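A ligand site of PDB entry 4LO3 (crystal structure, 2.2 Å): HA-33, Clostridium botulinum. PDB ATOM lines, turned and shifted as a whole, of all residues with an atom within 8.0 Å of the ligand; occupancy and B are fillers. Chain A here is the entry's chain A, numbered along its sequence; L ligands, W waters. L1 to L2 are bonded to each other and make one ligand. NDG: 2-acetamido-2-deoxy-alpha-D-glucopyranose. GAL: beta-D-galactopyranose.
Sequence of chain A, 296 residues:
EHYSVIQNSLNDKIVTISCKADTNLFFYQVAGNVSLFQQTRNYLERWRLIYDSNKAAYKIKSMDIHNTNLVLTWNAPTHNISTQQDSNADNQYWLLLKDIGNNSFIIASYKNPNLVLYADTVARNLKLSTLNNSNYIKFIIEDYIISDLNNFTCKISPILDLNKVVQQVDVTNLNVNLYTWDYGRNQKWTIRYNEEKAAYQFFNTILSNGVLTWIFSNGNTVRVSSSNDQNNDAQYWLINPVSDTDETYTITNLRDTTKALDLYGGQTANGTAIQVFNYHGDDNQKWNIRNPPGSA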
ATOM      1  N   ASN A 220     -18.215  24.919  -8.340  1.00  0.00           N
ATOM      2  CA  ASN A 220     -16.808  25.106  -8.715  1.00  0.00           C
ATOM      3  C   ASN A 220     -16.055  23.800  -9.004  1.00  0.00           C
ATOM      4  O   ASN A 220     -14.837  23.802  -9.205  1.00  0.00           O
ATOM      5  CB  ASN A 220     -16.080  25.868  -7.609  1.00  0.00           C
ATOM      6  CG  ASN A 220     -16.451  27.323  -7.560  1.00  0.00           C
ATOM      7  OD1 ASN A 220     -16.822  27.918  -8.579  1.00  0.00           O
ATOM      8  ND2 ASN A 220     -16.343  27.925  -6.386  1.00  0.00           N
ATOM      9  N   ALA A 260     -10.695  30.419 -12.743  1.00  0.00           N
ATOM     10  CA  ALA A 260      -9.336  29.903 -12.906  1.00  0.00           C
ATOM     11  C   ALA A 260      -9.124  28.579 -12.180  1.00  0.00           C
ATOM     12  O   ALA A 260      -9.669  28.376 -11.080  1.00  0.00           O
ATOM     13  CB  ALA A 260      -8.320  30.932 -12.417  1.00  0.00           C
ATOM     14  N   LEU A 261      -8.332  27.702 -12.783  1.00  0.00           N
ATOM     15  CA  LEU A 261      -7.920  26.464 -12.114  1.00  0.00           C
ATOM     16  C   LEU A 261      -7.290  26.787 -10.754  1.00  0.00           C
ATOM     17  O   LEU A 261      -6.363  27.615 -10.677  1.00  0.00           O
ATOM     18  CB  LEU A 261      -6.959  25.649 -12.979  1.00  0.00           C
ATOM     19  CG  LEU A 261      -6.880  24.165 -12.590  1.00  0.00           C
ATOM     20  CD1 LEU A 261      -8.236  23.479 -12.861  1.00  0.00           C
ATOM     21  CD2 LEU A 261      -5.744  23.448 -13.319  1.00  0.00           C
ATOM     22  N   ASP A 262      -7.791  26.145  -9.704  1.00  0.00           N
ATOM     23  CA  ASP A 262      -7.581  26.579  -8.329  1.00  0.00           C
ATOM     24  C   ASP A 262      -7.286  25.387  -7.411  1.00  0.00           C
ATOM     25  O   ASP A 262      -7.982  24.355  -7.455  1.00  0.00           O
ATOM     26  CB  ASP A 262      -8.854  27.309  -7.848  1.00  0.00           C
ATOM     27  CG  ASP A 262      -8.706  27.949  -6.485  1.00  0.00           C
ATOM     28  OD1 ASP A 262      -8.482  29.181  -6.421  1.00  0.00           O
ATOM     29  OD2 ASP A 262      -8.834  27.227  -5.460  1.00  0.00           O
ATOM     30  N   LEU A 263      -6.232  25.514  -6.601  1.00  0.00           N
ATOM     31  CA  LEU A 263      -5.917  24.498  -5.597  1.00  0.00           C
ATOM     32  C   LEU A 263      -6.582  24.888  -4.288  1.00  0.00           C
ATOM     33  O   LEU A 263      -6.244  25.912  -3.696  1.00  0.00           O
ATOM     34  CB  LEU A 263      -4.400  24.362  -5.392  1.00  0.00           C
ATOM     35  CG  LEU A 263      -3.989  23.401  -4.257  1.00  0.00           C
ATOM     36  CD1 LEU A 263      -4.509  21.993  -4.539  1.00  0.00           C
ATOM     37  CD2 LEU A 263      -2.482  23.397  -4.004  1.00  0.00           C
ATOM     38  N   TYR A 264      -7.538  24.073  -3.839  1.00  0.00           N
ATOM     39  CA  TYR A 264      -8.412  24.404  -2.707  1.00  0.00           C
ATOM     40  C   TYR A 264      -7.661  24.867  -1.473  1.00  0.00           C
ATOM     41  O   TYR A 264      -6.850  24.125  -0.906  1.00  0.00           O
ATOM     42  CB  TYR A 264      -9.319  23.229  -2.332  1.00  0.00           C
ATOM     43  CG  TYR A 264     -10.485  23.642  -1.464  1.00  0.00           C
ATOM     44  CD1 TYR A 264     -11.711  23.961  -2.024  1.00  0.00           C
ATOM     45  CD2 TYR A 264     -10.345  23.750  -0.074  1.00  0.00           C
ATOM     46  CE1 TYR A 264     -12.780  24.347  -1.239  1.00  0.00           C
ATOM     47  CE2 TYR A 264     -11.415  24.146   0.713  1.00  0.00           C
ATOM     48  CZ  TYR A 264     -12.629  24.451   0.130  1.00  0.00           C
ATOM     49  OH  TYR A 264     -13.704  24.839   0.906  1.00  0.00           O
ATOM     50  N   GLY A 265      -7.936  26.102  -1.057  1.00  0.00           N
ATOM     51  CA  GLY A 265      -7.358  26.668   0.145  1.00  0.00           C
ATOM     52  C   GLY A 265      -5.858  26.944   0.058  1.00  0.00           C
ATOM     53  O   GLY A 265      -5.277  27.492   0.996  1.00  0.00           O
ATOM     54  N   GLY A 266      -5.238  26.589  -1.066  1.00  0.00           N
ATOM     55  CA  GLY A 266      -3.791  26.532  -1.152  1.00  0.00           C
ATOM     56  C   GLY A 266      -3.249  25.380  -0.307  1.00  0.00           C
ATOM     57  O   GLY A 266      -2.062  25.354   0.060  1.00  0.00           O
ATOM     58  N   GLN A 267      -4.125  24.420  -0.004  1.00  0.00           N
ATOM     59  CA  GLN A 267      -3.771  23.257   0.807  1.00  0.00           C
ATOM     60  C   GLN A 267      -3.005  22.269  -0.061  1.00  0.00           C
ATOM     61  O   GLN A 267      -3.359  22.033  -1.222  1.00  0.00           O
ATOM     62  CB  GLN A 267      -5.022  22.612   1.394  1.00  0.00           C
ATOM     63  CG  GLN A 267      -5.875  23.545   2.260  1.00  0.00           C
ATOM     64  CD  GLN A 267      -5.149  24.022   3.515  1.00  0.00           C
ATOM     65  OE1 GLN A 267      -4.510  23.230   4.212  1.00  0.00           O
ATOM     66  NE2 GLN A 267      -5.253  25.318   3.803  1.00  0.00           N
ATOM     67  N   ALA A 273      -8.676  19.058  -3.064  1.00  0.00           N
ATOM     68  CA  ALA A 273      -9.480  19.245  -4.270  1.00  0.00           C
ATOM     69  C   ALA A 273      -8.868  20.215  -5.288  1.00  0.00           C
ATOM     70  O   ALA A 273      -8.315  21.256  -4.936  1.00  0.00           O
ATOM     71  CB  ALA A 273     -10.897  19.697  -3.898  1.00  0.00           C
ATOM     72  N   GLN A 275     -10.205  22.565  -8.344  1.00  0.00           N
ATOM     73  CA  GLN A 275     -11.502  23.128  -8.692  1.00  0.00           C
ATOM     74  C   GLN A 275     -11.271  24.344  -9.569  1.00  0.00           C
ATOM     75  O   GLN A 275     -10.136  24.602  -9.990  1.00  0.00           O
ATOM     76  CB  GLN A 275     -12.224  23.565  -7.420  1.00  0.00           C
ATOM     77  CG  GLN A 275     -11.493  24.700  -6.703  1.00  0.00           C
ATOM     78  CD  GLN A 275     -12.223  25.196  -5.462  1.00  0.00           C
ATOM     79  OE1 GLN A 275     -13.191  24.591  -4.984  1.00  0.00           O
ATOM     80  NE2 GLN A 275     -11.730  26.312  -4.918  1.00  0.00           N
ATOM     81  N   VAL A 276     -12.341  25.079  -9.864  1.00  0.00           N
ATOM     82  CA  VAL A 276     -12.178  26.426 -10.409  1.00  0.00           C
ATOM     83  C   VAL A 276     -12.614  27.426  -9.358  1.00  0.00           C
ATOM     84  O   VAL A 276     -13.338  27.087  -8.411  1.00  0.00           O
ATOM     85  CB  VAL A 276     -12.962  26.671 -11.715  1.00  0.00           C
ATOM     86  CG1 VAL A 276     -12.401  25.820 -12.844  1.00  0.00           C
ATOM     87  CG2 VAL A 276     -14.452  26.414 -11.495  1.00  0.00           C
ATOM     88  N   PHE A 277     -12.190  28.662  -9.527  1.00  0.00           N
ATOM     89  CA  PHE A 277     -12.491  29.711  -8.569  1.00  0.00           C
ATOM     90  C   PHE A 277     -12.235  31.046  -9.254  1.00  0.00           C
ATOM     91  O   PHE A 277     -11.515  31.110 -10.258  1.00  0.00           O
ATOM     92  CB  PHE A 277     -11.574  29.556  -7.347  1.00  0.00           C
ATOM     93  CG  PHE A 277     -12.035  30.321  -6.145  1.00  0.00           C
ATOM     94  CD1 PHE A 277     -12.968  29.775  -5.272  1.00  0.00           C
ATOM     95  CD2 PHE A 277     -11.529  31.596  -5.870  1.00  0.00           C
ATOM     96  CE1 PHE A 277     -13.392  30.478  -4.146  1.00  0.00           C
ATOM     97  CE2 PHE A 277     -11.945  32.301  -4.749  1.00  0.00           C
ATOM     98  CZ  PHE A 277     -12.878  31.745  -3.879  1.00  0.00           C
ATOM     99  N   ASN A 278     -12.850  32.116  -8.729  1.00  0.00           N
ATOM    100  CA  ASN A 278     -12.621  33.450  -9.249  1.00  0.00           C
ATOM    101  C   ASN A 278     -11.125  33.785  -9.284  1.00  0.00           C
ATOM    102  O   ASN A 278     -10.403  33.526  -8.307  1.00  0.00           O
ATOM    103  CB  ASN A 278     -13.386  34.489  -8.420  1.00  0.00           C
ATOM    104  CG  ASN A 278     -13.327  35.867  -9.023  1.00  0.00           C
ATOM    105  OD1 ASN A 278     -13.818  36.088 -10.140  1.00  0.00           O
ATOM    106  ND2 ASN A 278     -12.718  36.813  -8.312  1.00  0.00           N
ATOM    107  N   TYR A 279     -10.651  34.311 -10.414  1.00  0.00           N
ATOM    108  CA  TYR A 279      -9.230  34.579 -10.609  1.00  0.00           C
ATOM    109  C   TYR A 279      -8.735  35.744  -9.761  1.00  0.00           C
ATOM    110  O   TYR A 279      -9.282  36.846  -9.816  1.00  0.00           O
ATOM    111  CB  TYR A 279      -8.930  34.855 -12.091  1.00  0.00           C
ATOM    112  CG  TYR A 279      -7.484  35.240 -12.340  1.00  0.00           C
ATOM    113  CD1 TYR A 279      -6.488  34.282 -12.326  1.00  0.00           C
ATOM    114  CD2 TYR A 279      -7.132  36.562 -12.577  1.00  0.00           C
ATOM    115  CE1 TYR A 279      -5.162  34.625 -12.552  1.00  0.00           C
ATOM    116  CE2 TYR A 279      -5.807  36.915 -12.800  1.00  0.00           C
ATOM    117  CZ  TYR A 279      -4.832  35.936 -12.788  1.00  0.00           C
ATOM    118  OH  TYR A 279      -3.514  36.277 -13.008  1.00  0.00           O
ATOM    119  N   HIS A 280      -7.696  35.492  -8.962  1.00  0.00           N
ATOM    120  CA  HIS A 280      -7.023  36.553  -8.209  1.00  0.00           C
ATOM    121  C   HIS A 280      -5.517  36.543  -8.472  1.00  0.00           C
ATOM    122  O   HIS A 280      -4.807  37.497  -8.111  1.00  0.00           O
ATOM    123  CB  HIS A 280      -7.325  36.450  -6.712  1.00  0.00           C
ATOM    124  CG  HIS A 280      -7.294  35.058  -6.161  1.00  0.00           C
ATOM    125  ND1 HIS A 280      -6.160  34.259  -6.182  1.00  0.00           N
ATOM    126  CD2 HIS A 280      -8.266  34.319  -5.562  1.00  0.00           C
ATOM    127  CE1 HIS A 280      -6.438  33.100  -5.628  1.00  0.00           C
ATOM    128  NE2 HIS A 280      -7.701  33.103  -5.249  1.00  0.00           N
ATOM    129  N   GLY A 281      -5.037  35.485  -9.112  1.00  0.00           N
ATOM    130  CA  GLY A 281      -3.629  35.379  -9.465  1.00  0.00           C
ATOM    131  C   GLY A 281      -2.707  35.054  -8.307  1.00  0.00           C
ATOM    132  O   GLY A 281      -1.493  35.269  -8.410  1.00  0.00           O
ATOM    133  N   ASP A 282      -3.247  34.541  -7.203  1.00  0.00           N
ATOM    134  CA  ASP A 282      -2.405  34.138  -6.081  1.00  0.00           C
ATOM    135  C   ASP A 282      -1.725  32.805  -6.400  1.00  0.00           C
ATOM    136  O   ASP A 282      -2.038  32.175  -7.416  1.00  0.00           O
ATOM    137  CB  ASP A 282      -3.194  34.050  -4.779  1.00  0.00           C
ATOM    138  CG  ASP A 282      -3.828  35.383  -4.368  1.00  0.00           C
ATOM    139  OD1 ASP A 282      -3.259  36.445  -4.723  1.00  0.00           O
ATOM    140  OD2 ASP A 282      -4.885  35.364  -3.692  1.00  0.00           O
ATOM    141  N   ASN A 284      -1.935  29.783  -5.385  1.00  0.00           N
ATOM    142  CA  ASN A 284      -2.756  28.574  -5.529  1.00  0.00           C
ATOM    143  C   ASN A 284      -3.569  28.550  -6.836  1.00  0.00           C
ATOM    144  O   ASN A 284      -4.412  27.675  -7.041  1.00  0.00           O
ATOM    145  CB  ASN A 284      -3.689  28.392  -4.333  1.00  0.00           C
ATOM    146  CG  ASN A 284      -4.811  29.414  -4.297  1.00  0.00           C
ATOM    147  OD1 ASN A 284      -4.582  30.609  -4.502  1.00  0.00           O
ATOM    148  ND2 ASN A 284      -6.029  28.953  -4.035  1.00  0.00           N
ATOM    149  N   GLN A 285      -3.326  29.519  -7.714  1.00  0.00           N
ATOM    150  CA  GLN A 285      -3.915  29.514  -9.059  1.00  0.00           C
ATOM    151  C   GLN A 285      -2.794  29.496 -10.118  1.00  0.00           C
ATOM    152  O   GLN A 285      -3.020  29.784 -11.290  1.00  0.00           O
ATOM    153  CB  GLN A 285      -4.855  30.708  -9.268  1.00  0.00           C
ATOM    154  CG  GLN A 285      -5.987  30.810  -8.219  1.00  0.00           C
ATOM    155  CD  GLN A 285      -7.076  31.830  -8.587  1.00  0.00           C
ATOM    156  OE1 GLN A 285      -6.810  32.800  -9.296  1.00  0.00           O
ATOM    157  NE2 GLN A 285      -8.299  31.599  -8.088  1.00  0.00           N
HETATM  158  C1  NDG L   1      -8.995  30.765   4.679  1.00  0.00           C
HETATM  159  C2  NDG L   1      -9.499  29.504   4.014  1.00  0.00           C
HETATM  160  C3  NDG L   1      -8.933  29.357   2.665  1.00  0.00           C
HETATM  161  C4  NDG L   1      -9.153  30.510   1.834  1.00  0.00           C
HETATM  162  C5  NDG L   1      -8.786  31.849   2.536  1.00  0.00           C
HETATM  163  C6  NDG L   1      -9.241  33.083   1.834  1.00  0.00           C
HETATM  164  C7  NDG L   1     -10.052  27.316   5.134  1.00  0.00           C
HETATM  165  C8  NDG L   1      -9.636  26.176   6.031  1.00  0.00           C
HETATM  166  O5  NDG L   1      -9.311  31.942   3.858  1.00  0.00           O
HETATM  167  O3  NDG L   1      -9.599  28.309   2.020  1.00  0.00           O
HETATM  168  O4  NDG L   1      -8.373  30.334   0.641  1.00  0.00           O
HETATM  169  O6  NDG L   1      -8.281  34.058   1.612  1.00  0.00           O
HETATM  170  O7  NDG L   1     -11.177  27.345   4.640  1.00  0.00           O
HETATM  171  N2  NDG L   1      -9.117  28.394   4.867  1.00  0.00           N
HETATM  172  O1  NDG L   1      -7.655  30.703   4.971  1.00  0.00           O
HETATM  173  C1  GAL L   2      -9.231  30.253  -0.488  1.00  0.00           C
HETATM  174  C2  GAL L   2      -8.484  30.538  -1.757  1.00  0.00           C
HETATM  175  C3  GAL L   2      -9.338  30.379  -2.905  1.00  0.00           C
HETATM  176  C4  GAL L   2      -9.995  29.068  -2.938  1.00  0.00           C
HETATM  177  C5  GAL L   2     -10.796  28.879  -1.648  1.00  0.00           C
HETATM  178  C6  GAL L   2     -11.599  27.539  -1.674  1.00  0.00           C
HETATM  179  O2  GAL L   2      -8.084  31.881  -1.777  1.00  0.00           O
HETATM  180  O3  GAL L   2      -8.538  30.605  -4.051  1.00  0.00           O
HETATM  181  O4  GAL L   2      -8.995  28.121  -3.047  1.00  0.00           O
HETATM  182  O5  GAL L   2      -9.989  28.978  -0.518  1.00  0.00           O
HETATM  183  O6  GAL L   2     -12.741  27.511  -2.439  1.00  0.00           O
HETATM  184  O   HOH W   1     -15.401  26.301  -4.343  1.00  0.00           O
HETATM  185  O   HOH W   2      -5.323  32.253  -2.233  1.00  0.00           O
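Water W2 lies within hydrogen-bond range of an oxygen (O2) of GAL L2 (2.8 Å), the side-chain amide oxygen (OD1) of Asn 284 (2.9 Å) and the side-chain carboxylate (OD2) of Asp 282 (3.5 Å). Water W1 lies within hydrogen-bond range of ND2 of Asn 220 (2.8 Å), OE1 of Gln 275 (2.9 Å) and O6 of GAL L2 (3.5 Å).
N of Gly 265 is in hydrogen-bond range of O4 of GAL L2, at 3.0 Å. The side-chain carboxylate (OD2) of Asp 262 sits at hydrogen-bond distance from an oxygen (O4) of GAL L2 (2.6 Å). A ring nitrogen (NE2) of His 280 sits at hydrogen-bond distance from an oxygen (O3) of GAL L2, 2.9 Å away. The side-chain amide nitrogen (NE2) of Gln 275 is in hydrogen-bond range of an oxygen (O6) of GAL L2 (2.9 Å). O3 of GAL L2 is in hydrogen-bond range of ND2 of Asn 284 (3.0 Å).
Residues that only touch the ligand: Leu 263 (3.6 Å), Tyr 264 (3.4 Å) and Phe 277 (3.5 Å). Hydrophobic or aromatic side chains that line the ligand: Tyr 264, Phe 277 and His 280.
The backbone carbonyl oxygen (O) of Phe 277 is in hydrogen-bond range of the backbone NH (N) of Ala 260 (2.7 Å). OE1 of Gln 285 sits at hydrogen-bond distance from N of His 280, at 2.9 Å. OD2 of Asp 282 is in hydrogen-bond range of ND1 of His 280. N of Tyr 264 sits at hydrogen-bond distance from O of Ala 273 (3.1 Å). The side-chain carboxylate of Asp 262 sits at hydrogen-bond distance from the side-chain amide nitrogen of Gln 285, 2.9 Å away. The backbone NH (N) of Asp 262 sits at hydrogen-bond distance from the backbone carbonyl oxygen (O) of Gln 275, at 2.8 Å. The backbone carbonyl oxygen (O) of Asn 284 lies within hydrogen-bond range of the backbone NH (N) of Leu 263. The side-chain amide nitrogen (ND2) of Asn 284 is in hydrogen-bond range of the side-chain carboxylate (OD1) of Asp 262, at 3.4 Å.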
